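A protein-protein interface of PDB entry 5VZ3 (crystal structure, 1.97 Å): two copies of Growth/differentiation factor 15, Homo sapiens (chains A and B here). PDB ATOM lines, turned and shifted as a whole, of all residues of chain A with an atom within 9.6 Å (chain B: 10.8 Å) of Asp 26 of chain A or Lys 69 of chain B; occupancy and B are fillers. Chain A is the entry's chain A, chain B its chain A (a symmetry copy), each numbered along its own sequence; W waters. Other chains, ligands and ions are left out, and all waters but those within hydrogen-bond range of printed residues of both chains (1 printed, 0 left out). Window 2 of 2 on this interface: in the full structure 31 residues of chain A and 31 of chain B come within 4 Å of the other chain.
Among the printed residues, pairs that only touch across the chains: Val 20 of chain A with Lys 69 of chain B, Arg 21 of chain A with Lys 69 of chain B, Ala 22 of chain A with Leu 65 of chain B, Asp 26 of chain A with Ser 64 of chain B, Asp 26 of chain A with Leu 68 of chain B, Leu 27 of chain A with Ile 61 of chain B, Leu 27 of chain A with Ser 64 of chain B, Trp 29 of chain A with Ile 61 of chain B, Val 41 of chain A with Ile 61 of chain B, Met 43 of chain A with Lys 62 of chain B, Met 43 of chain A with Leu 65 of chain B, Met 43 of chain A with Val 73 of chain B, Ile 45 of chain A with Thr 72 of chain B and Ile 45 of chain A with Pro 74 of chain B.
Water W1 bridges O of Leu 27 of chain A and OG of Ser 64 of chain B.
No position is printed for both chains. Of the 15 pairs that touch across the chains among the printed residues, none has its exchanged pair printed and touching as well.
The side-chain carboxylate of Asp 26 of chain A lies within salt-bridge range of the side-chain amino group of Lys 69 of chain B (3.95 Å).
OG of Ser 23 of chain A is in hydrogen-bond range of N of Asp 26 of chain A. O of Val 20 of chain A sits at hydrogen-bond distance from N of Val 41 of chain A (2.7 Å). The backbone NH (N) of Trp 29 of chain A is in hydrogen-bond range of the backbone carbonyl oxygen (O) of Leu 24 of chain A, at 2.9 Å. O of Ala 22 of chain A sits at hydrogen-bond distance from N of Val 39 of chain A. ND1 of His 66 of chain B lies within hydrogen-bond range of O of Val 73 of chain B, at 2.7 Å. OG of Ser 64 of chain B lies within hydrogen-bond range of O of Gln 60 of chain B (3.2 Å).
Hydrophobic or aromatic side chains of chain A within 4 Å of the printed part of chain B: Val 20, Ala 22, Leu 27, Trp 29, Val 41, Met 43 and Ile 45. Along chain A the printed residues that touch a printed residue of chain B span positions 20 to 45. Printed residues of chain B that touch a printed residue of chain A: Ile 61, Lys 62, Ser 64, Leu 65, Leu 68, Lys 69, Thr 72, Val 73 and Pro 74. Hydrophobic or aromatic side chains of chain B within 4 Å of the printed part of chain A: Ile 61, Leu 65, Leu 68, Val 73 and Pro 74. Among the printed residues, Asp or Glu carboxylates within 4 Å of a Lys or Arg side-chain nitrogen of the other chain: Asp 26 of chain A with Lys 69 of chain B (3.95 Å).
Ala 22 of chain A touches just one residue of chain B: Leu 65. No residue of chain B comes within 4 Å of Ser 23 of chain A. Of chain B, only Ser 64, Leu 68 and Lys 69 come within 4 Å of Asp 26 of chain A. Of chain B, only Ile 61 and Ser 64 come within 4 Å of Leu 27 of chain A. Asp 31 of chain A touches none of the printed residues of chain B. Of the printed residues of chain B, Val 41 of chain A touches Ile 61 (3.97 Å). Of the printed residues of chain A, Lys 62 of chain B touches Met 43 (3.97 Å). Leu 65 of chain B touches just these residues of chain A: Ala 22 (3.9 Å) and Met 43 (3.9 Å). Of the printed residues of chain A, Lys 69 of chain B touches Val 20 (3.7 Å), Arg 21 (3.9 Å) and Asp 26 (3.95 Å). Of the printed residues of chain A, Val 73 of chain B touches Met 43 (3.6 Å).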
ATOM      1  N   THR A  19      -4.841   3.751 -28.001  1.00  0.00           N
ATOM      2  CA  THR A  19      -3.538   3.901 -28.666  1.00  0.00           C
ATOM      3  C   THR A  19      -2.523   4.290 -27.647  1.00  0.00           C
ATOM      4  O   THR A  19      -2.730   5.206 -26.879  1.00  0.00           O
ATOM      5  CB  THR A  19      -3.614   4.952 -29.745  1.00  0.00           C
ATOM      6  OG1 THR A  19      -4.632   4.511 -30.625  1.00  0.00           O
ATOM      7  CG2 THR A  19      -2.236   5.050 -30.508  1.00  0.00           C
ATOM      8  N   VAL A  20      -1.447   3.528 -27.553  1.00  0.00           N
ATOM      9  CA  VAL A  20      -0.407   3.830 -26.603  1.00  0.00           C
ATOM     10  C   VAL A  20       0.837   4.062 -27.478  1.00  0.00           C
ATOM     11  O   VAL A  20       1.191   3.184 -28.290  1.00  0.00           O
ATOM     12  CB  VAL A  20      -0.153   2.664 -25.634  1.00  0.00           C
ATOM     13  CG1 VAL A  20       1.018   2.999 -24.702  1.00  0.00           C
ATOM     14  CG2 VAL A  20      -1.445   2.409 -24.816  1.00  0.00           C
ATOM     15  N   ARG A  21       1.488   5.212 -27.298  1.00  0.00           N
ATOM     16  CA  ARG A  21       2.683   5.591 -28.111  1.00  0.00           C
ATOM     17  C   ARG A  21       3.893   5.071 -27.439  1.00  0.00           C
ATOM     18  O   ARG A  21       4.025   5.220 -26.269  1.00  0.00           O
ATOM     19  CB  ARG A  21       2.773   7.100 -28.286  1.00  0.00           C
ATOM     20  CG  ARG A  21       1.963   7.538 -29.497  1.00  0.00           C
ATOM     21  CD  ARG A  21       1.540   9.018 -29.491  1.00  0.00           C
ATOM     22  NE  ARG A  21       0.449   9.198 -30.465  1.00  0.00           N
ATOM     23  CZ  ARG A  21      -0.847   8.934 -30.244  1.00  0.00           C
ATOM     24  NH1 ARG A  21      -1.299   8.514 -29.050  1.00  0.00           N
ATOM     25  NH2 ARG A  21      -1.713   9.095 -31.241  1.00  0.00           N
ATOM     26  N   ALA A  22       4.736   4.355 -28.163  1.00  0.00           N
ATOM     27  CA  ALA A  22       5.848   3.684 -27.552  1.00  0.00           C
ATOM     28  C   ALA A  22       7.079   3.861 -28.440  1.00  0.00           C
ATOM     29  O   ALA A  22       7.045   3.587 -29.643  1.00  0.00           O
ATOM     30  CB  ALA A  22       5.547   2.196 -27.375  1.00  0.00           C
ATOM     31  N   SER A  23       8.173   4.224 -27.821  1.00  0.00           N
ATOM     32  CA  SER A  23       9.451   4.215 -28.545  1.00  0.00           C
ATOM     33  C   SER A  23       9.998   2.804 -28.650  1.00  0.00           C
ATOM     34  O   SER A  23       9.664   1.909 -27.855  1.00  0.00           O
ATOM     35  CB  SER A  23      10.468   5.104 -27.854  1.00  0.00           C
ATOM     36  OG  SER A  23      10.992   4.505 -26.693  1.00  0.00           O
ATOM     37  N   LEU A  24      10.940   2.635 -29.564  1.00  0.00           N
ATOM     38  CA  LEU A  24      11.653   1.415 -29.697  1.00  0.00           C
ATOM     39  C   LEU A  24      12.350   1.049 -28.441  1.00  0.00           C
ATOM     40  O   LEU A  24      12.409  -0.128 -28.132  1.00  0.00           O
ATOM     41  CB  LEU A  24      12.634   1.461 -30.864  1.00  0.00           C
ATOM     42  CG  LEU A  24      11.939   1.533 -32.208  1.00  0.00           C
ATOM     43  CD1 LEU A  24      12.997   1.610 -33.321  1.00  0.00           C
ATOM     44  CD2 LEU A  24      10.972   0.427 -32.435  1.00  0.00           C
ATOM     45  N   GLU A  25      12.848   2.035 -27.678  1.00  0.00           N
ATOM     46  CA  GLU A  25      13.600   1.737 -26.465  1.00  0.00           C
ATOM     47  C   GLU A  25      12.584   1.250 -25.369  1.00  0.00           C
ATOM     48  O   GLU A  25      12.895   0.397 -24.568  1.00  0.00           O
ATOM     49  CB  GLU A  25      14.400   2.994 -25.996  1.00  0.00           C
ATOM     50  CG  GLU A  25      15.509   3.475 -26.970  1.00  0.00           C
ATOM     51  CD  GLU A  25      15.046   4.218 -28.282  1.00  0.00           C
ATOM     52  OE1 GLU A  25      15.949   4.498 -29.139  1.00  0.00           O
ATOM     53  OE2 GLU A  25      13.824   4.551 -28.500  1.00  0.00           O
ATOM     54  N   ASP A  26      11.388   1.830 -25.377  1.00  0.00           N
ATOM     55  CA  ASP A  26      10.251   1.385 -24.517  1.00  0.00           C
ATOM     56  C   ASP A  26       9.941  -0.120 -24.753  1.00  0.00           C
ATOM     57  O   ASP A  26       9.731  -0.865 -23.811  1.00  0.00           O
ATOM     58  CB  ASP A  26       8.981   2.185 -24.835  1.00  0.00           C
ATOM     59  CG  ASP A  26       9.046   3.663 -24.359  1.00  0.00           C
ATOM     60  OD1 ASP A  26       9.949   3.958 -23.552  1.00  0.00           O
ATOM     61  OD2 ASP A  26       8.200   4.506 -24.820  1.00  0.00           O
ATOM     62  N   LEU A  27       9.952  -0.535 -26.016  1.00  0.00           N
ATOM     63  CA  LEU A  27       9.565  -1.900 -26.418  1.00  0.00           C
ATOM     64  C   LEU A  27      10.644  -2.886 -26.251  1.00  0.00           C
ATOM     65  O   LEU A  27      10.423  -4.094 -26.362  1.00  0.00           O
ATOM     66  CB  LEU A  27       9.115  -1.902 -27.879  1.00  0.00           C
ATOM     67  CG  LEU A  27       7.920  -1.054 -28.105  1.00  0.00           C
ATOM     68  CD1 LEU A  27       7.460  -1.030 -29.530  1.00  0.00           C
ATOM     69  CD2 LEU A  27       6.755  -1.505 -27.227  1.00  0.00           C
ATOM     70  N   GLY A  28      11.859  -2.389 -26.050  1.00  0.00           N
ATOM     71  CA  GLY A  28      13.014  -3.250 -26.021  1.00  0.00           C
ATOM     72  C   GLY A  28      13.454  -3.648 -27.432  1.00  0.00           C
ATOM     73  O   GLY A  28      14.206  -4.577 -27.560  1.00  0.00           O
ATOM     74  N   TRP A  29      13.015  -2.919 -28.461  1.00  0.00           N
ATOM     75  CA  TRP A  29      13.309  -3.255 -29.834  1.00  0.00           C
ATOM     76  C   TRP A  29      14.486  -2.472 -30.470  1.00  0.00           C
ATOM     77  O   TRP A  29      14.819  -2.740 -31.603  1.00  0.00           O
ATOM     78  CB  TRP A  29      12.102  -3.036 -30.685  1.00  0.00           C
ATOM     79  CG  TRP A  29      10.966  -3.959 -30.398  1.00  0.00           C
ATOM     80  CD1 TRP A  29      10.946  -5.040 -29.548  1.00  0.00           C
ATOM     81  CD2 TRP A  29       9.704  -3.878 -30.975  1.00  0.00           C
ATOM     82  NE1 TRP A  29       9.694  -5.593 -29.515  1.00  0.00           N
ATOM     83  CE2 TRP A  29       8.908  -4.912 -30.402  1.00  0.00           C
ATOM     84  CE3 TRP A  29       9.139  -3.040 -31.947  1.00  0.00           C
ATOM     85  CZ2 TRP A  29       7.608  -5.135 -30.774  1.00  0.00           C
ATOM     86  CZ3 TRP A  29       7.828  -3.255 -32.331  1.00  0.00           C
ATOM     87  CH2 TRP A  29       7.060  -4.317 -31.721  1.00  0.00           C
ATOM     88  N   ALA A  30      15.113  -1.551 -29.766  1.00  0.00           N
ATOM     89  CA  ALA A  30      15.961  -0.552 -30.437  1.00  0.00           C
ATOM     90  C   ALA A  30      17.227  -1.188 -31.079  1.00  0.00           C
ATOM     91  O   ALA A  30      17.688  -0.697 -32.087  1.00  0.00           O
ATOM     92  CB  ALA A  30      16.299   0.621 -29.493  1.00  0.00           C
ATOM     93  N   ASP A  31      17.725  -2.309 -30.551  1.00  0.00           N
ATOM     94  CA  ASP A  31      18.874  -3.013 -31.198  1.00  0.00           C
ATOM     95  C   ASP A  31      18.597  -3.573 -32.572  1.00  0.00           C
ATOM     96  O   ASP A  31      19.515  -3.730 -33.335  1.00  0.00           O
ATOM     97  CB  ASP A  31      19.355  -4.248 -30.407  1.00  0.00           C
ATOM     98  CG  ASP A  31      19.942  -3.920 -29.066  1.00  0.00           C
ATOM     99  OD1 ASP A  31      20.436  -2.787 -28.859  1.00  0.00           O
ATOM    100  OD2 ASP A  31      19.918  -4.842 -28.224  1.00  0.00           O
ATOM    101  N   ARG A  37      10.300   4.475 -35.552  1.00  0.00           N
ATOM    102  CA  ARG A  37      11.039   4.707 -34.320  1.00  0.00           C
ATOM    103  C   ARG A  37      10.034   4.947 -33.180  1.00  0.00           C
ATOM    104  O   ARG A  37      10.401   4.815 -32.019  1.00  0.00           O
ATOM    105  CB  ARG A  37      12.009   5.911 -34.456  1.00  0.00           C
ATOM    106  CG  ARG A  37      13.304   5.676 -35.262  1.00  0.00           C
ATOM    107  CD  ARG A  37      13.188   5.841 -36.799  1.00  0.00           C
ATOM    108  NE  ARG A  37      12.639   7.120 -37.326  1.00  0.00           N
ATOM    109  CZ  ARG A  37      13.333   8.210 -37.726  1.00  0.00           C
ATOM    110  NH1 ARG A  37      14.673   8.286 -37.654  1.00  0.00           N
ATOM    111  NH2 ARG A  37      12.669   9.266 -38.199  1.00  0.00           N
ATOM    112  N   GLU A  38       8.817   5.290 -33.523  1.00  0.00           N
ATOM    113  CA  GLU A  38       7.723   5.480 -32.563  1.00  0.00           C
ATOM    114  C   GLU A  38       6.629   4.576 -33.029  1.00  0.00           C
ATOM    115  O   GLU A  38       6.221   4.668 -34.173  1.00  0.00           O
ATOM    116  CB  GLU A  38       7.270   6.956 -32.619  1.00  0.00           C
ATOM    117  CG  GLU A  38       6.324   7.434 -31.523  1.00  0.00           C
ATOM    118  CD  GLU A  38       6.968   7.531 -30.135  1.00  0.00           C
ATOM    119  OE1 GLU A  38       8.149   7.114 -29.925  1.00  0.00           O
ATOM    120  OE2 GLU A  38       6.251   8.050 -29.237  1.00  0.00           O
ATOM    121  N   VAL A  39       6.127   3.699 -32.157  1.00  0.00           N
ATOM    122  CA  VAL A  39       4.993   2.831 -32.523  1.00  0.00           C
ATOM    123  C   VAL A  39       3.713   3.280 -31.834  1.00  0.00           C
ATOM    124  O   VAL A  39       3.706   3.570 -30.635  1.00  0.00           O
ATOM    125  CB  VAL A  39       5.287   1.331 -32.222  1.00  0.00           C
ATOM    126  CG1 VAL A  39       4.180   0.439 -32.788  1.00  0.00           C
ATOM    127  CG2 VAL A  39       6.651   0.907 -32.778  1.00  0.00           C
ATOM    128  N   VAL A  41       0.802   1.866 -30.641  1.00  0.00           N
ATOM    129  CA  VAL A  41       0.359   0.507 -30.312  1.00  0.00           C
ATOM    130  C   VAL A  41      -1.130   0.569 -29.998  1.00  0.00           C
ATOM    131  O   VAL A  41      -1.541   1.172 -29.009  1.00  0.00           O
ATOM    132  CB  VAL A  41       1.097  -0.038 -29.109  1.00  0.00           C
ATOM    133  CG1 VAL A  41       0.601  -1.499 -28.849  1.00  0.00           C
ATOM    134  CG2 VAL A  41       2.609  -0.028 -29.323  1.00  0.00           C
ATOM    135  N   MET A  43      -4.166  -1.094 -28.347  1.00  0.00           N
ATOM    136  CA  MET A  43      -4.417  -2.105 -27.339  1.00  0.00           C
ATOM    137  C   MET A  43      -5.734  -1.957 -26.624  1.00  0.00           C
ATOM    138  O   MET A  43      -6.336  -0.882 -26.592  1.00  0.00           O
ATOM    139  CB  MET A  43      -3.251  -2.257 -26.337  1.00  0.00           C
ATOM    140  CG  MET A  43      -2.936  -1.148 -25.385  1.00  0.00           C
ATOM    141  SD  MET A  43      -1.744  -1.868 -24.159  1.00  0.00           S
ATOM    142  CE  MET A  43      -0.271  -1.739 -25.101  1.00  0.00           C
ATOM    143  N   ILE A  45      -7.937  -1.946 -23.488  1.00  0.00           N
ATOM    144  CA  ILE A  45      -7.809  -1.575 -22.103  1.00  0.00           C
ATOM    145  C   ILE A  45      -9.191  -1.120 -21.595  1.00  0.00           C
ATOM    146  O   ILE A  45      -9.921  -0.433 -22.308  1.00  0.00           O
ATOM    147  CB  ILE A  45      -6.812  -0.375 -21.935  1.00  0.00           C
ATOM    148  CG1 ILE A  45      -5.491  -0.578 -22.654  1.00  0.00           C
ATOM    149  CG2 ILE A  45      -6.463  -0.224 -20.462  1.00  0.00           C
ATOM    150  CD1 ILE A  45      -4.497   0.576 -22.404  1.00  0.00           C
ATOM    151  N   MET B  57       3.128 -11.660 -29.970  1.00  0.00           N
ATOM    152  CA  MET B  57       3.993 -10.539 -29.746  1.00  0.00           C
ATOM    153  C   MET B  57       3.280  -9.403 -29.081  1.00  0.00           C
ATOM    154  O   MET B  57       3.935  -8.685 -28.370  1.00  0.00           O
ATOM    155  CB  MET B  57       4.635 -10.065 -31.058  1.00  0.00           C
ATOM    156  CG  MET B  57       5.732 -10.990 -31.584  1.00  0.00           C
ATOM    157  SD  MET B  57       6.451 -10.381 -33.148  1.00  0.00           S
ATOM    158  CE  MET B  57       7.588  -9.085 -32.613  1.00  0.00           C
ATOM    159  N   ALA B  59       1.334  -9.625 -26.597  1.00  0.00           N
ATOM    160  CA  ALA B  59       1.490  -9.924 -25.169  1.00  0.00           C
ATOM    161  C   ALA B  59       2.818  -9.463 -24.628  1.00  0.00           C
ATOM    162  O   ALA B  59       2.907  -8.929 -23.507  1.00  0.00           O
ATOM    163  CB  ALA B  59       1.341 -11.391 -24.932  1.00  0.00           C
ATOM    164  N   GLN B  60       3.873  -9.652 -25.411  1.00  0.00           N
ATOM    165  CA  GLN B  60       5.201  -9.175 -25.019  1.00  0.00           C
ATOM    166  C   GLN B  60       5.317  -7.679 -24.910  1.00  0.00           C
ATOM    167  O   GLN B  60       5.957  -7.156 -23.987  1.00  0.00           O
ATOM    168  CB  GLN B  60       6.239  -9.735 -26.027  1.00  0.00           C
ATOM    169  CG  GLN B  60       6.267 -11.282 -26.005  1.00  0.00           C
ATOM    170  CD  GLN B  60       7.021 -11.937 -27.190  1.00  0.00           C
ATOM    171  OE1 GLN B  60       6.875 -11.540 -28.361  1.00  0.00           O
ATOM    172  NE2 GLN B  60       7.826 -12.953 -26.879  1.00  0.00           N
ATOM    173  N   ILE B  61       4.696  -6.992 -25.858  1.00  0.00           N
ATOM    174  CA  ILE B  61       4.563  -5.564 -25.852  1.00  0.00           C
ATOM    175  C   ILE B  61       3.816  -5.081 -24.615  1.00  0.00           C
ATOM    176  O   ILE B  61       4.284  -4.179 -23.911  1.00  0.00           O
ATOM    177  CB  ILE B  61       3.839  -5.075 -27.097  1.00  0.00           C
ATOM    178  CG1 ILE B  61       4.748  -5.237 -28.310  1.00  0.00           C
ATOM    179  CG2 ILE B  61       3.428  -3.606 -27.018  1.00  0.00           C
ATOM    180  CD1 ILE B  61       3.997  -4.993 -29.608  1.00  0.00           C
ATOM    181  N   LYS B  62       2.681  -5.691 -24.302  1.00  0.00           N
ATOM    182  CA  LYS B  62       1.984  -5.367 -23.070  1.00  0.00           C
ATOM    183  C   LYS B  62       2.816  -5.555 -21.806  1.00  0.00           C
ATOM    184  O   LYS B  62       2.748  -4.751 -20.915  1.00  0.00           O
ATOM    185  CB  LYS B  62       0.706  -6.167 -22.946  1.00  0.00           C
ATOM    186  CG  LYS B  62      -0.380  -5.574 -23.787  1.00  0.00           C
ATOM    187  CD  LYS B  62      -1.610  -6.477 -23.767  1.00  0.00           C
ATOM    188  CE  LYS B  62      -2.465  -6.263 -22.534  1.00  0.00           C
ATOM    189  NZ  LYS B  62      -3.449  -7.408 -22.424  1.00  0.00           N
ATOM    190  N   THR B  63       3.581  -6.610 -21.714  1.00  0.00           N
ATOM    191  CA  THR B  63       4.523  -6.781 -20.649  1.00  0.00           C
ATOM    192  C   THR B  63       5.524  -5.617 -20.518  1.00  0.00           C
ATOM    193  O   THR B  63       5.766  -5.122 -19.394  1.00  0.00           O
ATOM    194  CB  THR B  63       5.311  -8.077 -20.822  1.00  0.00           C
ATOM    195  OG1 THR B  63       4.419  -9.177 -20.710  1.00  0.00           O
ATOM    196  CG2 THR B  63       6.364  -8.215 -19.741  1.00  0.00           C
ATOM    197  N   SER B  64       6.109  -5.212 -21.653  1.00  0.00           N
ATOM    198  CA  SER B  64       7.071  -4.136 -21.672  1.00  0.00           C
ATOM    199  C   SER B  64       6.439  -2.814 -21.242  1.00  0.00           C
ATOM    200  O   SER B  64       6.967  -2.109 -20.418  1.00  0.00           O
ATOM    201  CB  SER B  64       7.667  -4.040 -23.051  1.00  0.00           C
ATOM    202  OG  SER B  64       8.362  -5.237 -23.305  1.00  0.00           O
ATOM    203  N   LEU B  65       5.284  -2.513 -21.762  1.00  0.00           N
ATOM    204  CA  LEU B  65       4.665  -1.239 -21.527  1.00  0.00           C
ATOM    205  C   LEU B  65       3.989  -1.193 -20.220  1.00  0.00           C
ATOM    206  O   LEU B  65       3.895  -0.119 -19.679  1.00  0.00           O
ATOM    207  CB  LEU B  65       3.689  -0.868 -22.633  1.00  0.00           C
ATOM    208  CG  LEU B  65       4.401  -0.694 -23.976  1.00  0.00           C
ATOM    209  CD1 LEU B  65       3.337  -0.343 -25.004  1.00  0.00           C
ATOM    210  CD2 LEU B  65       5.505   0.381 -23.894  1.00  0.00           C
ATOM    211  N   HIS B  66       3.467  -2.323 -19.733  1.00  0.00           N
ATOM    212  CA  HIS B  66       2.946  -2.412 -18.358  1.00  0.00           C
ATOM    213  C   HIS B  66       4.050  -2.029 -17.294  1.00  0.00           C
ATOM    214  O   HIS B  66       3.777  -1.290 -16.354  1.00  0.00           O
ATOM    215  CB  HIS B  66       2.376  -3.794 -18.003  1.00  0.00           C
ATOM    216  CG  HIS B  66       1.998  -3.901 -16.562  1.00  0.00           C
ATOM    217  ND1 HIS B  66       1.002  -3.131 -15.986  1.00  0.00           N
ATOM    218  CD2 HIS B  66       2.544  -4.621 -15.555  1.00  0.00           C
ATOM    219  CE1 HIS B  66       0.929  -3.410 -14.696  1.00  0.00           C
ATOM    220  NE2 HIS B  66       1.844  -4.312 -14.418  1.00  0.00           N
ATOM    221  N   ARG B  67       5.262  -2.558 -17.441  1.00  0.00           N
ATOM    222  CA  ARG B  67       6.382  -2.179 -16.573  1.00  0.00           C
ATOM    223  C   ARG B  67       6.656  -0.642 -16.573  1.00  0.00           C
ATOM    224  O   ARG B  67       6.925  -0.008 -15.549  1.00  0.00           O
ATOM    225  CB  ARG B  67       7.623  -2.936 -17.025  1.00  0.00           C
ATOM    226  CG  ARG B  67       8.854  -2.643 -16.177  1.00  0.00           C
ATOM    227  CD  ARG B  67      10.031  -3.498 -16.572  1.00  0.00           C
ATOM    228  NE  ARG B  67      11.262  -2.914 -16.056  1.00  0.00           N
ATOM    229  CZ  ARG B  67      11.962  -1.901 -16.594  1.00  0.00           C
ATOM    230  NH1 ARG B  67      11.602  -1.288 -17.712  1.00  0.00           N
ATOM    231  NH2 ARG B  67      13.042  -1.465 -15.956  1.00  0.00           N
ATOM    232  N   LEU B  68       6.610  -0.046 -17.735  1.00  0.00           N
ATOM    233  CA  LEU B  68       6.881   1.372 -17.841  1.00  0.00           C
ATOM    234  C   LEU B  68       5.761   2.330 -17.562  1.00  0.00           C
ATOM    235  O   LEU B  68       6.038   3.463 -17.187  1.00  0.00           O
ATOM    236  CB  LEU B  68       7.425   1.672 -19.236  1.00  0.00           C
ATOM    237  CG  LEU B  68       8.741   1.006 -19.540  1.00  0.00           C
ATOM    238  CD1 LEU B  68       9.149   1.316 -20.972  1.00  0.00           C
ATOM    239  CD2 LEU B  68       9.833   1.414 -18.559  1.00  0.00           C
ATOM    240  N   LYS B  69       4.512   1.900 -17.764  1.00  0.00           N
ATOM    241  CA  LYS B  69       3.310   2.704 -17.567  1.00  0.00           C
ATOM    242  C   LYS B  69       2.196   1.914 -16.880  1.00  0.00           C
ATOM    243  O   LYS B  69       1.103   1.691 -17.453  1.00  0.00           O
ATOM    244  CB  LYS B  69       2.770   3.227 -18.890  1.00  0.00           C
ATOM    245  CG  LYS B  69       3.761   3.750 -19.850  1.00  0.00           C
ATOM    246  CD  LYS B  69       2.998   4.114 -21.138  1.00  0.00           C
ATOM    247  CE  LYS B  69       3.808   3.876 -22.406  1.00  0.00           C
ATOM    248  NZ  LYS B  69       4.976   4.789 -22.548  1.00  0.00           N
ATOM    249  N   PRO B  70       2.449   1.472 -15.653  1.00  0.00           N
ATOM    250  CA  PRO B  70       1.559   0.591 -14.968  1.00  0.00           C
ATOM    251  C   PRO B  70       0.205   1.169 -14.578  1.00  0.00           C
ATOM    252  O   PRO B  70      -0.664   0.412 -14.324  1.00  0.00           O
ATOM    253  CB  PRO B  70       2.344   0.170 -13.730  1.00  0.00           C
ATOM    254  CG  PRO B  70       3.328   1.269 -13.531  1.00  0.00           C
ATOM    255  CD  PRO B  70       3.662   1.778 -14.862  1.00  0.00           C
ATOM    256  N   ASP B  71       0.027   2.472 -14.548  1.00  0.00           N
ATOM    257  CA  ASP B  71      -1.280   3.024 -14.252  1.00  0.00           C
ATOM    258  C   ASP B  71      -2.107   3.143 -15.519  1.00  0.00           C
ATOM    259  O   ASP B  71      -3.312   3.394 -15.443  1.00  0.00           O
ATOM    260  CB  ASP B  71      -1.130   4.423 -13.645  1.00  0.00           C
ATOM    261  CG  ASP B  71      -0.456   4.401 -12.276  1.00  0.00           C
ATOM    262  OD1 ASP B  71      -0.657   3.456 -11.467  1.00  0.00           O
ATOM    263  OD2 ASP B  71       0.275   5.361 -12.021  1.00  0.00           O
ATOM    264  N   THR B  72      -1.441   3.018 -16.646  1.00  0.00           N
ATOM    265  CA  THR B  72      -2.033   3.168 -17.962  1.00  0.00           C
ATOM    266  C   THR B  72      -2.250   1.813 -18.663  1.00  0.00           C
ATOM    267  O   THR B  72      -3.308   1.536 -19.197  1.00  0.00           O
ATOM    268  CB  THR B  72      -1.077   4.057 -18.792  1.00  0.00           C
ATOM    269  OG1 THR B  72      -1.099   5.361 -18.237  1.00  0.00           O
ATOM    270  CG2 THR B  72      -1.469   4.151 -20.315  1.00  0.00           C
ATOM    271  N   VAL B  73      -1.188   1.034 -18.761  1.00  0.00           N
ATOM    272  CA  VAL B  73      -1.147  -0.243 -19.478  1.00  0.00           C
ATOM    273  C   VAL B  73      -1.214  -1.428 -18.516  1.00  0.00           C
ATOM    274  O   VAL B  73      -0.368  -1.573 -17.671  1.00  0.00           O
ATOM    275  CB  VAL B  73       0.118  -0.399 -20.318  1.00  0.00           C
ATOM    276  CG1 VAL B  73       0.124  -1.754 -21.065  1.00  0.00           C
ATOM    277  CG2 VAL B  73       0.173   0.704 -21.349  1.00  0.00           C
ATOM    278  N   PRO B  74      -2.248  -2.288 -18.647  1.00  0.00           N
ATOM    279  CA  PRO B  74      -2.373  -3.449 -17.773  1.00  0.00           C
ATOM    280  C   PRO B  74      -1.384  -4.572 -18.203  1.00  0.00           C
ATOM    281  O   PRO B  74      -0.985  -4.623 -19.392  1.00  0.00           O
ATOM    282  CB  PRO B  74      -3.820  -3.900 -18.081  1.00  0.00           C
ATOM    283  CG  PRO B  74      -3.985  -3.614 -19.558  1.00  0.00           C
ATOM    284  CD  PRO B  74      -3.257  -2.292 -19.741  1.00  0.00           C
ATOM    285  N   ALA B  75      -0.975  -5.424 -17.272  1.00  0.00           N
ATOM    286  CA  ALA B  75      -0.287  -6.714 -17.616  1.00  0.00           C
ATOM    287  C   ALA B  75      -1.075  -7.630 -18.592  1.00  0.00           C
ATOM    288  O   ALA B  75      -2.283  -7.518 -18.677  1.00  0.00           O
ATOM    289  CB  ALA B  75      -0.035  -7.476 -16.343  1.00  0.00           C
ATOM    290  N   PRO B  76      -0.398  -8.542 -19.310  1.00  0.00           N
ATOM    291  CA  PRO B  76      -1.171  -9.593 -19.964  1.00  0.00           C
ATOM    292  C   PRO B  76      -2.034 -10.364 -18.971  1.00  0.00           C
ATOM    293  O   PRO B  76      -1.680 -10.507 -17.812  1.00  0.00           O
ATOM    294  CB  PRO B  76      -0.106 -10.496 -20.590  1.00  0.00           C
ATOM    295  CG  PRO B  76       1.103  -9.672 -20.625  1.00  0.00           C
ATOM    296  CD  PRO B  76       1.046  -8.746 -19.484  1.00  0.00           C
HETATM  297  O   HOH W   1       8.171  -5.388 -26.074  1.00  0.00           O
